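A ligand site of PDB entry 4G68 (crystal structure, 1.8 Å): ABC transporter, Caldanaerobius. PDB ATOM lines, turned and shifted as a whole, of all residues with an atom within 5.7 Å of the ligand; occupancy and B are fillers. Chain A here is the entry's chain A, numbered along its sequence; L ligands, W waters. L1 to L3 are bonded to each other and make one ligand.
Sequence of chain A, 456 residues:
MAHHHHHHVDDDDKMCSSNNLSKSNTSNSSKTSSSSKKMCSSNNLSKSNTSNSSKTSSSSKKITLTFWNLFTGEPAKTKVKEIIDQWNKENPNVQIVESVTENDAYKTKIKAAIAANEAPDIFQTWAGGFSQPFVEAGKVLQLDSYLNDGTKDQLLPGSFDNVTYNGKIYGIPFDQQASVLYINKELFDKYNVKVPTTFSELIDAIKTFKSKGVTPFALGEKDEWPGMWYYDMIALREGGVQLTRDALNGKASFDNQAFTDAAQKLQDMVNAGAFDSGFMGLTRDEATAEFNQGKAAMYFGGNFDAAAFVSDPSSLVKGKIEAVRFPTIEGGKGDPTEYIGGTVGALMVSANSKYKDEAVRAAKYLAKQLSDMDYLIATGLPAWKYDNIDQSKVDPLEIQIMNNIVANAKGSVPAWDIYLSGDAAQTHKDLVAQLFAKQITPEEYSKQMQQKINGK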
ATOM      1  N   LEU A  70      15.423 -11.995  32.059  1.00  0.00           N
ATOM      2  CA  LEU A  70      15.106 -11.709  30.670  1.00  0.00           C
ATOM      3  C   LEU A  70      16.271 -11.757  29.749  1.00  0.00           C
ATOM      4  O   LEU A  70      16.198 -11.179  28.674  1.00  0.00           O
ATOM      5  CB  LEU A  70      14.339 -10.341  30.622  1.00  0.00           C
ATOM      6  CG  LEU A  70      15.080  -9.109  31.233  1.00  0.00           C
ATOM      7  CD1 LEU A  70      16.481  -8.844  30.643  1.00  0.00           C
ATOM      8  CD2 LEU A  70      14.237  -7.891  30.858  1.00  0.00           C
ATOM      9  N   PHE A  71      17.419 -12.330  30.201  1.00  0.00           N
ATOM     10  CA  PHE A  71      18.584 -12.325  29.329  1.00  0.00           C
ATOM     11  C   PHE A  71      18.503 -13.363  28.201  1.00  0.00           C
ATOM     12  O   PHE A  71      18.988 -14.490  28.307  1.00  0.00           O
ATOM     13  CB  PHE A  71      19.857 -12.466  30.133  1.00  0.00           C
ATOM     14  CG  PHE A  71      20.166 -11.216  30.948  1.00  0.00           C
ATOM     15  CD1 PHE A  71      20.650 -10.051  30.324  1.00  0.00           C
ATOM     16  CD2 PHE A  71      19.855 -11.185  32.316  1.00  0.00           C
ATOM     17  CE1 PHE A  71      20.909  -8.891  31.101  1.00  0.00           C
ATOM     18  CE2 PHE A  71      20.076 -10.030  33.050  1.00  0.00           C
ATOM     19  CZ  PHE A  71      20.594  -8.889  32.455  1.00  0.00           C
ATOM     20  N   THR A  72      17.849 -12.967  27.126  1.00  0.00           N
ATOM     21  CA  THR A  72      17.538 -13.876  26.051  1.00  0.00           C
ATOM     22  C   THR A  72      18.569 -13.870  24.916  1.00  0.00           C
ATOM     23  O   THR A  72      18.710 -14.839  24.261  1.00  0.00           O
ATOM     24  CB  THR A  72      16.153 -13.629  25.396  1.00  0.00           C
ATOM     25  OG1 THR A  72      15.955 -12.252  25.138  1.00  0.00           O
ATOM     26  CG2 THR A  72      15.000 -14.209  26.251  1.00  0.00           C
ATOM     27  N   GLY A  73      19.203 -12.737  24.699  1.00  0.00           N
ATOM     28  CA  GLY A  73      20.184 -12.634  23.647  1.00  0.00           C
ATOM     29  C   GLY A  73      21.591 -13.168  23.985  1.00  0.00           C
ATOM     30  O   GLY A  73      21.893 -13.326  25.137  1.00  0.00           O
ATOM     31  N   GLU A  74      22.419 -13.411  22.967  1.00  0.00           N
ATOM     32  CA  GLU A  74      23.805 -13.908  23.157  1.00  0.00           C
ATOM     33  C   GLU A  74      24.765 -12.687  23.135  1.00  0.00           C
ATOM     34  O   GLU A  74      24.518 -11.740  22.418  1.00  0.00           O
ATOM     35  CB  GLU A  74      24.180 -14.897  22.022  1.00  0.00           C
ATOM     36  CG  GLU A  74      23.324 -16.153  22.079  1.00  0.00           C
ATOM     37  CD  GLU A  74      23.639 -17.081  23.262  1.00  0.00           C
ATOM     38  OE1 GLU A  74      24.532 -16.779  24.139  1.00  0.00           O
ATOM     39  OE2 GLU A  74      22.970 -18.148  23.345  1.00  0.00           O
ATOM     40  N   ALA A  76      24.780 -12.992  26.520  1.00  0.00           N
ATOM     41  CA  ALA A  76      24.220 -12.994  27.894  1.00  0.00           C
ATOM     42  C   ALA A  76      23.558 -14.303  28.239  1.00  0.00           C
ATOM     43  O   ALA A  76      23.779 -14.825  29.315  1.00  0.00           O
ATOM     44  CB  ALA A  76      23.304 -11.800  28.157  1.00  0.00           C
ATOM     45  N   LYS A  77      22.764 -14.881  27.312  1.00  0.00           N
ATOM     46  CA  LYS A  77      22.043 -16.098  27.682  1.00  0.00           C
ATOM     47  C   LYS A  77      23.073 -17.182  28.112  1.00  0.00           C
ATOM     48  O   LYS A  77      22.874 -17.839  29.162  1.00  0.00           O
ATOM     49  CB  LYS A  77      21.198 -16.581  26.478  1.00  0.00           C
ATOM     50  CG  LYS A  77      20.445 -17.903  26.710  1.00  0.00           C
ATOM     51  CD  LYS A  77      19.825 -18.316  25.352  1.00  0.00           C
ATOM     52  CE  LYS A  77      19.329 -19.757  25.372  1.00  0.00           C
ATOM     53  NZ  LYS A  77      18.382 -20.037  26.497  1.00  0.00           N
ATOM     54  N   ASN A 103      12.259  -9.685  27.288  1.00  0.00           N
ATOM     55  CA  ASN A 103      11.877  -8.422  27.942  1.00  0.00           C
ATOM     56  C   ASN A 103      10.407  -8.064  28.011  1.00  0.00           C
ATOM     57  O   ASN A 103       9.826  -7.989  29.108  1.00  0.00           O
ATOM     58  CB  ASN A 103      12.726  -7.308  27.268  1.00  0.00           C
ATOM     59  CG  ASN A 103      12.466  -5.914  27.809  1.00  0.00           C
ATOM     60  OD1 ASN A 103      12.359  -5.710  29.001  1.00  0.00           O
ATOM     61  ND2 ASN A 103      12.419  -4.922  26.917  1.00  0.00           N
ATOM     62  N   ASP A 104       9.803  -7.751  26.852  1.00  0.00           N
ATOM     63  CA  ASP A 104       8.415  -7.244  26.956  1.00  0.00           C
ATOM     64  C   ASP A 104       7.429  -8.339  27.415  1.00  0.00           C
ATOM     65  O   ASP A 104       6.497  -8.070  28.207  1.00  0.00           O
ATOM     66  CB  ASP A 104       8.019  -6.540  25.678  1.00  0.00           C
ATOM     67  CG  ASP A 104       8.577  -5.155  25.633  1.00  0.00           C
ATOM     68  OD1 ASP A 104       8.198  -4.356  26.528  1.00  0.00           O
ATOM     69  OD2 ASP A 104       9.496  -4.963  24.850  1.00  0.00           O
ATOM     70  N   LYS A 107       7.736  -8.693  31.360  1.00  0.00           N
ATOM     71  CA  LYS A 107       6.882  -7.787  32.162  1.00  0.00           C
ATOM     72  C   LYS A 107       5.513  -8.384  32.405  1.00  0.00           C
ATOM     73  O   LYS A 107       5.031  -8.392  33.560  1.00  0.00           O
ATOM     74  CB  LYS A 107       6.667  -6.481  31.391  1.00  0.00           C
ATOM     75  CG  LYS A 107       7.994  -5.803  31.122  1.00  0.00           C
ATOM     76  CD  LYS A 107       7.795  -4.650  30.114  1.00  0.00           C
ATOM     77  CE  LYS A 107       9.176  -4.066  29.881  1.00  0.00           C
ATOM     78  NZ  LYS A 107       9.166  -3.036  28.734  1.00  0.00           N
ATOM     79  N   GLN A 124      14.137 -11.136  38.408  1.00  0.00           N
ATOM     80  CA  GLN A 124      14.693  -9.877  37.942  1.00  0.00           C
ATOM     81  C   GLN A 124      13.574  -8.847  37.868  1.00  0.00           C
ATOM     82  O   GLN A 124      12.432  -9.209  37.628  1.00  0.00           O
ATOM     83  CB  GLN A 124      15.325 -10.078  36.583  1.00  0.00           C
ATOM     84  CG  GLN A 124      15.974  -8.861  35.974  1.00  0.00           C
ATOM     85  CD  GLN A 124      16.558  -9.102  34.579  1.00  0.00           C
ATOM     86  OE1 GLN A 124      16.654 -10.226  34.138  1.00  0.00           O
ATOM     87  NE2 GLN A 124      17.066  -8.036  33.939  1.00  0.00           N
ATOM     88  N   TRP A 126      12.650  -4.275  37.670  1.00  0.00           N
ATOM     89  CA  TRP A 126      13.055  -2.880  37.577  1.00  0.00           C
ATOM     90  C   TRP A 126      12.648  -2.194  38.840  1.00  0.00           C
ATOM     91  O   TRP A 126      11.484  -2.216  39.225  1.00  0.00           O
ATOM     92  CB  TRP A 126      12.364  -2.169  36.370  1.00  0.00           C
ATOM     93  CG  TRP A 126      12.898  -2.754  35.050  1.00  0.00           C
ATOM     94  CD1 TRP A 126      14.060  -2.445  34.356  1.00  0.00           C
ATOM     95  CD2 TRP A 126      12.284  -3.807  34.303  1.00  0.00           C
ATOM     96  NE1 TRP A 126      14.192  -3.224  33.234  1.00  0.00           N
ATOM     97  CE2 TRP A 126      13.127  -4.033  33.128  1.00  0.00           C
ATOM     98  CE3 TRP A 126      11.102  -4.552  34.459  1.00  0.00           C
ATOM     99  CZ2 TRP A 126      12.850  -5.006  32.212  1.00  0.00           C
ATOM    100  CZ3 TRP A 126      10.787  -5.509  33.486  1.00  0.00           C
ATOM    101  CH2 TRP A 126      11.635  -5.688  32.366  1.00  0.00           C
ATOM    102  N   ASP A 175      22.306  -3.620  38.441  1.00  0.00           N
ATOM    103  CA  ASP A 175      22.719  -2.720  37.295  1.00  0.00           C
ATOM    104  C   ASP A 175      22.108  -1.325  37.243  1.00  0.00           C
ATOM    105  O   ASP A 175      21.070  -1.057  37.897  1.00  0.00           O
ATOM    106  CB  ASP A 175      22.858  -3.421  35.906  1.00  0.00           C
ATOM    107  CG  ASP A 175      21.537  -3.727  35.223  1.00  0.00           C
ATOM    108  OD1 ASP A 175      20.494  -3.262  35.595  1.00  0.00           O
ATOM    109  OD2 ASP A 175      21.562  -4.514  34.235  1.00  0.00           O
ATOM    110  N   GLN A 177      21.202   2.028  34.563  1.00  0.00           N
ATOM    111  CA  GLN A 177      20.906   2.352  33.177  1.00  0.00           C
ATOM    112  C   GLN A 177      21.348   3.805  32.894  1.00  0.00           C
ATOM    113  O   GLN A 177      21.442   4.627  33.809  1.00  0.00           O
ATOM    114  CB  GLN A 177      19.384   2.251  32.954  1.00  0.00           C
ATOM    115  CG  GLN A 177      18.924   0.769  32.980  1.00  0.00           C
ATOM    116  CD  GLN A 177      17.474   0.641  32.558  1.00  0.00           C
ATOM    117  OE1 GLN A 177      16.778   1.655  32.312  1.00  0.00           O
ATOM    118  NE2 GLN A 177      16.984  -0.613  32.512  1.00  0.00           N
ATOM    119  N   TRP A 225       8.163   1.327  24.440  1.00  0.00           N
ATOM    120  CA  TRP A 225       9.120   1.885  25.371  1.00  0.00           C
ATOM    121  C   TRP A 225      10.445   2.409  24.683  1.00  0.00           C
ATOM    122  O   TRP A 225      10.972   3.376  25.120  1.00  0.00           O
ATOM    123  CB  TRP A 225       9.359   0.888  26.534  1.00  0.00           C
ATOM    124  CG  TRP A 225      10.095  -0.333  26.126  1.00  0.00           C
ATOM    125  CD1 TRP A 225       9.584  -1.578  25.753  1.00  0.00           C
ATOM    126  CD2 TRP A 225      11.552  -0.416  25.945  1.00  0.00           C
ATOM    127  NE1 TRP A 225      10.583  -2.423  25.362  1.00  0.00           N
ATOM    128  CE2 TRP A 225      11.818  -1.763  25.458  1.00  0.00           C
ATOM    129  CE3 TRP A 225      12.648   0.519  26.097  1.00  0.00           C
ATOM    130  CZ2 TRP A 225      13.131  -2.221  25.202  1.00  0.00           C
ATOM    131  CZ3 TRP A 225      13.972   0.029  25.786  1.00  0.00           C
ATOM    132  CH2 TRP A 225      14.201  -1.331  25.347  1.00  0.00           C
ATOM    133  N   MET A 228       9.672   5.900  23.495  1.00  0.00           N
ATOM    134  CA  MET A 228       9.460   6.682  24.694  1.00  0.00           C
ATOM    135  C   MET A 228      10.747   7.206  25.275  1.00  0.00           C
ATOM    136  O   MET A 228      10.707   8.310  25.787  1.00  0.00           O
ATOM    137  CB  MET A 228       8.727   5.836  25.720  1.00  0.00           C
ATOM    138  CG  MET A 228       8.222   6.583  26.914  1.00  0.00           C
ATOM    139  SD  MET A 228       8.168   5.230  28.421  1.00  0.00           S
ATOM    140  CE  MET A 228      10.153   4.949  28.392  1.00  0.00           C
ATOM    141  N   TRP A 229      11.833   6.459  25.272  1.00  0.00           N
ATOM    142  CA  TRP A 229      13.123   7.026  25.687  1.00  0.00           C
ATOM    143  C   TRP A 229      13.483   8.302  25.009  1.00  0.00           C
ATOM    144  O   TRP A 229      14.039   9.232  25.664  1.00  0.00           O
ATOM    145  CB  TRP A 229      14.261   6.028  25.518  1.00  0.00           C
ATOM    146  CG  TRP A 229      14.338   5.049  26.652  1.00  0.00           C
ATOM    147  CD1 TRP A 229      13.346   4.155  27.136  1.00  0.00           C
ATOM    148  CD2 TRP A 229      15.488   4.837  27.527  1.00  0.00           C
ATOM    149  NE1 TRP A 229      13.836   3.467  28.205  1.00  0.00           N
ATOM    150  CE2 TRP A 229      15.107   3.847  28.498  1.00  0.00           C
ATOM    151  CE3 TRP A 229      16.775   5.406  27.605  1.00  0.00           C
ATOM    152  CZ2 TRP A 229      16.002   3.377  29.499  1.00  0.00           C
ATOM    153  CZ3 TRP A 229      17.651   4.958  28.616  1.00  0.00           C
ATOM    154  CH2 TRP A 229      17.267   3.964  29.545  1.00  0.00           C
ATOM    155  N   ARG A 284      12.630  -3.593  19.411  1.00  0.00           N
ATOM    156  CA  ARG A 284      14.011  -3.214  19.817  1.00  0.00           C
ATOM    157  C   ARG A 284      15.014  -4.111  19.213  1.00  0.00           C
ATOM    158  O   ARG A 284      16.000  -3.645  18.704  1.00  0.00           O
ATOM    159  CB  ARG A 284      14.120  -3.236  21.348  1.00  0.00           C
ATOM    160  CG  ARG A 284      15.445  -2.701  21.960  1.00  0.00           C
ATOM    161  CD  ARG A 284      16.470  -3.847  22.053  1.00  0.00           C
ATOM    162  NE  ARG A 284      15.941  -4.894  22.944  1.00  0.00           N
ATOM    163  CZ  ARG A 284      16.166  -5.006  24.264  1.00  0.00           C
ATOM    164  NH1 ARG A 284      16.950  -4.115  24.924  1.00  0.00           N
ATOM    165  NH2 ARG A 284      15.633  -6.056  24.933  1.00  0.00           N
ATOM    166  N   ASP A 285      14.827  -5.427  19.375  1.00  0.00           N
ATOM    167  CA  ASP A 285      15.785  -6.382  18.789  1.00  0.00           C
ATOM    168  C   ASP A 285      15.965  -6.247  17.268  1.00  0.00           C
ATOM    169  O   ASP A 285      17.076  -6.388  16.732  1.00  0.00           O
ATOM    170  CB  ASP A 285      15.355  -7.829  19.147  1.00  0.00           C
ATOM    171  CG  ASP A 285      15.486  -8.143  20.656  1.00  0.00           C
ATOM    172  OD1 ASP A 285      16.155  -7.419  21.437  1.00  0.00           O
ATOM    173  OD2 ASP A 285      14.949  -9.142  21.075  1.00  0.00           O
ATOM    174  N   PHE A 304      22.131  -0.564  27.794  1.00  0.00           N
ATOM    175  CA  PHE A 304      22.020  -2.025  27.780  1.00  0.00           C
ATOM    176  C   PHE A 304      22.079  -2.631  26.386  1.00  0.00           C
ATOM    177  O   PHE A 304      22.375  -3.837  26.227  1.00  0.00           O
ATOM    178  CB  PHE A 304      20.783  -2.539  28.538  1.00  0.00           C
ATOM    179  CG  PHE A 304      19.546  -1.706  28.287  1.00  0.00           C
ATOM    180  CD1 PHE A 304      18.853  -1.729  27.057  1.00  0.00           C
ATOM    181  CD2 PHE A 304      19.095  -0.867  29.276  1.00  0.00           C
ATOM    182  CE1 PHE A 304      17.712  -0.903  26.845  1.00  0.00           C
ATOM    183  CE2 PHE A 304      17.988  -0.031  29.078  1.00  0.00           C
ATOM    184  CZ  PHE A 304      17.288  -0.060  27.869  1.00  0.00           C
ATOM    185  N   ASP A 305      21.755  -1.786  25.405  1.00  0.00           N
ATOM    186  CA  ASP A 305      21.807  -2.130  23.995  1.00  0.00           C
ATOM    187  C   ASP A 305      23.235  -2.216  23.442  1.00  0.00           C
ATOM    188  O   ASP A 305      23.476  -2.742  22.321  1.00  0.00           O
ATOM    189  CB  ASP A 305      20.899  -1.257  23.171  1.00  0.00           C
ATOM    190  CG  ASP A 305      19.387  -1.562  23.415  1.00  0.00           C
ATOM    191  OD1 ASP A 305      19.024  -2.641  23.889  1.00  0.00           O
ATOM    192  OD2 ASP A 305      18.587  -0.679  23.180  1.00  0.00           O
ATOM    193  N   ALA A 307      25.683  -4.093  24.165  1.00  0.00           N
ATOM    194  CA  ALA A 307      26.029  -5.422  23.769  1.00  0.00           C
ATOM    195  C   ALA A 307      25.649  -5.855  22.386  1.00  0.00           C
ATOM    196  O   ALA A 307      26.456  -6.607  21.758  1.00  0.00           O
ATOM    197  CB  ALA A 307      25.478  -6.465  24.809  1.00  0.00           C
ATOM    198  N   THR A 379      26.102  -5.385  28.473  1.00  0.00           N
ATOM    199  CA  THR A 379      24.660  -5.500  28.559  1.00  0.00           C
ATOM    200  C   THR A 379      24.134  -4.644  29.719  1.00  0.00           C
ATOM    201  O   THR A 379      22.935  -4.533  29.915  1.00  0.00           O
ATOM    202  CB  THR A 379      24.229  -6.967  28.853  1.00  0.00           C
ATOM    203  OG1 THR A 379      25.070  -7.510  29.840  1.00  0.00           O
ATOM    204  CG2 THR A 379      24.362  -7.835  27.595  1.00  0.00           C
ATOM    205  N   ALA A 415      13.664   6.012  33.145  1.00  0.00           N
ATOM    206  CA  ALA A 415      12.655   6.106  32.054  1.00  0.00           C
ATOM    207  C   ALA A 415      11.254   6.061  32.646  1.00  0.00           C
ATOM    208  O   ALA A 415      11.033   5.408  33.667  1.00  0.00           O
ATOM    209  CB  ALA A 415      12.851   4.942  31.142  1.00  0.00           C
ATOM    210  N   ASP A 417       8.420   4.770  32.133  1.00  0.00           N
ATOM    211  CA  ASP A 417       7.624   3.529  32.340  1.00  0.00           C
ATOM    212  C   ASP A 417       8.207   2.591  33.419  1.00  0.00           C
ATOM    213  O   ASP A 417       7.569   1.555  33.706  1.00  0.00           O
ATOM    214  CB  ASP A 417       7.477   2.738  31.045  1.00  0.00           C
ATOM    215  CG  ASP A 417       8.835   2.155  30.535  1.00  0.00           C
ATOM    216  OD1 ASP A 417       9.931   2.637  30.963  1.00  0.00           O
ATOM    217  OD2 ASP A 417       8.777   1.193  29.718  1.00  0.00           O
ATOM    218  N   ILE A 418       9.324   2.983  34.048  1.00  0.00           N
ATOM    219  CA  ILE A 418       9.845   2.334  35.232  1.00  0.00           C
ATOM    220  C   ILE A 418       9.528   3.246  36.442  1.00  0.00           C
ATOM    221  O   ILE A 418       9.469   2.814  37.559  1.00  0.00           O
ATOM    222  CB  ILE A 418      11.421   2.259  35.185  1.00  0.00           C
ATOM    223  CG1 ILE A 418      11.902   1.439  34.065  1.00  0.00           C
ATOM    224  CG2 ILE A 418      12.046   1.790  36.522  1.00  0.00           C
ATOM    225  CD1 ILE A 418      13.438   1.317  34.064  1.00  0.00           C
HETATM  226  C1  LIG L   1      20.129  -9.545  26.624  1.00  0.00           C
HETATM  227  C2  LIG L   1      18.608  -9.265  26.552  1.00  0.00           C
HETATM  228  C3  LIG L   1      18.211  -7.799  26.721  1.00  0.00           C
HETATM  229  C4  LIG L   1      19.023  -7.146  27.865  1.00  0.00           C
HETATM  230  C5  LIG L   1      20.514  -7.347  27.613  1.00  0.00           C
HETATM  231  O1  LIG L   1      20.648 -10.347  25.624  1.00  0.00           O
HETATM  232  O2  LIG L   1      17.943  -9.800  25.470  1.00  0.00           O
HETATM  233  O3  LIG L   1      16.845  -7.765  26.953  1.00  0.00           O
HETATM  234  O4  LIG L   1      18.635  -5.837  28.203  1.00  0.00           O
HETATM  235  O5  LIG L   1      20.939  -8.465  26.976  1.00  0.00           O
HETATM  236  C1  LG2 L   2      17.519  -5.564  28.794  1.00  0.00           C
HETATM  237  C2  LG2 L   2      17.906  -4.766  30.038  1.00  0.00           C
HETATM  238  C3  LG2 L   2      16.570  -4.314  30.675  1.00  0.00           C
HETATM  239  C4  LG2 L   2      15.880  -3.477  29.631  1.00  0.00           C
HETATM  240  C5  LG2 L   2      15.659  -4.300  28.342  1.00  0.00           C
HETATM  241  O1  LG2 L   2      18.557  -5.667  30.926  1.00  0.00           O
HETATM  242  O2  LG2 L   2      16.987  -3.456  31.761  1.00  0.00           O
HETATM  243  O3  LG2 L   2      14.606  -3.121  30.193  1.00  0.00           O
HETATM  244  O4  LG2 L   2      16.943  -4.705  27.866  1.00  0.00           O
HETATM  245  C1  LG3 L   3      14.020  -1.922  29.796  1.00  0.00           C
HETATM  246  C2  LG3 L   3      12.509  -2.054  29.982  1.00  0.00           C
HETATM  247  C3  LG3 L   3      11.882  -0.689  29.647  1.00  0.00           C
HETATM  248  C4  LG3 L   3      12.582   0.475  30.396  1.00  0.00           C
HETATM  249  C5  LG3 L   3      14.132   0.397  30.315  1.00  0.00           C
HETATM  250  O1  LG3 L   3      12.038  -3.105  29.170  1.00  0.00           O
HETATM  251  O2  LG3 L   3      10.488  -0.795  29.991  1.00  0.00           O
HETATM  252  O3  LG3 L   3      12.159   1.760  29.921  1.00  0.00           O
HETATM  253  O4  LG3 L   3      14.567  -0.922  30.633  1.00  0.00           O
HETATM  254  O   HOH W   1       7.256  -0.988  29.495  1.00  0.00           O
HETATM  255  O   HOH W   2      23.546 -10.314  25.277  1.00  0.00           O
HETATM  256  O   HOH W   3      15.029  -9.814  26.421  1.00  0.00           O
HETATM  257  O   HOH W   4       9.622  -1.976  32.507  1.00  0.00           O
HETATM  258  O   HOH W   5      18.325  -4.227  33.984  1.00  0.00           O
HETATM  259  O   HOH W   6      20.852  -4.517  31.665  1.00  0.00           O
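O of Leu 70 touches C2 of LIG L1, 3.7 Å away.
CD1 of Phe 71 touches O5 of LIG L1 (3.7 Å).
Ala 76 touches the ligand.
CD2 of Trp 225 touches C3 of LG3 L3 (3.7 Å).
CD1 of Phe 304 touches O4 of LG2 L2, 3.6 Å away.
CG2 of Thr 379 touches O5 of LIG L1, at 3.5 Å.
Ala 415 touches the ligand.
Ile 418 touches the ligand.
Hydrophobic or aromatic side chains that line the ligand: Leu 70, Phe 71, Ala 76, Trp 126, Trp 225, Trp 229, Phe 304, Ala 415 and Ile 418.
Along chain A the residues within 4 Å of the ligand span positions 70 to 418.
O3 of LG3 L3 is in hydrogen-bond range of OD1 of Asp 417.
The side-chain amide oxygen (OD1) of Asn 103 sits at hydrogen-bond distance from an oxygen (O1) of LG3 L3.
An oxygen (O2) of LG3 L3 sits at hydrogen-bond distance from the side-chain amino group of Lys 107 (2.9 Å).
NH2 of Arg 284 sits at hydrogen-bond distance from O3 of LIG L1.
The side-chain amide nitrogen (NE2) of Gln 177 is in hydrogen-bond range of an oxygen (O2) of LG2 L2 (2.9 Å).
O1 of LIG L1 lies within hydrogen-bond range of N of Gly 73.
The backbone carbonyl oxygen of Gly 73 lies close to an oxygen (O1) of LIG L1 (3.3 Å).
An oxygen (O3) of LG3 L3 lies within hydrogen-bond range of the indole nitrogen (NE1) of Trp 229 (2.9 Å).
The indole nitrogen (NE1) of Trp 126 is in hydrogen-bond range of an oxygen (O3) of LG2 L2 (3.1 Å).
OG1 of Thr 72 is in hydrogen-bond range of O2 of LIG L1, 3.2 Å away.
The side-chain sulfur (SD) of Met 228 sits close to the backbone NH (N) of Asp 417 (3.7 Å).
ND2 of Asn 103 sits close to NE1 of Trp 225 (3.5 Å).
The side-chain amino group (NZ) of Lys 107 is in salt-bridge range of the side-chain carboxylate (OD1) of Asp 104 (2.7 Å).
The guanidinium group of Arg 284 lies within salt-bridge range of the side-chain carboxylate of Asp 305, 2.7 Å away.
The guanidinium group (NE) of Arg 284 lies within salt-bridge range of the side-chain carboxylate (OD1) of Asp 285, at 2.9 Å.
OD2 of Asp 104 lies within hydrogen-bond range of NE1 of Trp 225 (2.8 Å).
OE1 of Gln 124 lies within hydrogen-bond range of N of Leu 70 (3.0 Å).
Water W6 lies within hydrogen-bond range of the side-chain carboxylate of Asp 175, an oxygen (O1) of LG2 L2 and the backbone carbonyl oxygen of Thr 379.
Water W5 bridges O2 of LG2 L2 and OD1 of Asp 175.
Water W3 lies within hydrogen-bond range of O3 of LIG L1 (2.8 Å), O of Leu 70 (2.9 Å), N of Asn 103 (2.9 Å) and OG1 of Thr 72 (2.9 Å).
Water W2 lies within hydrogen-bond range of an oxygen (O1) of LIG L1, the backbone NH of Ala 76, the backbone carbonyl oxygen of Glu 74 and the backbone carbonyl oxygen of Gly 73.
Water W1 lies within hydrogen-bond range of the side-chain carboxylate of Asp 417 (2.7 Å), the side-chain amino group of Lys 107 (2.9 Å) and an oxygen (O2) of LG3 L3 (3.3 Å).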
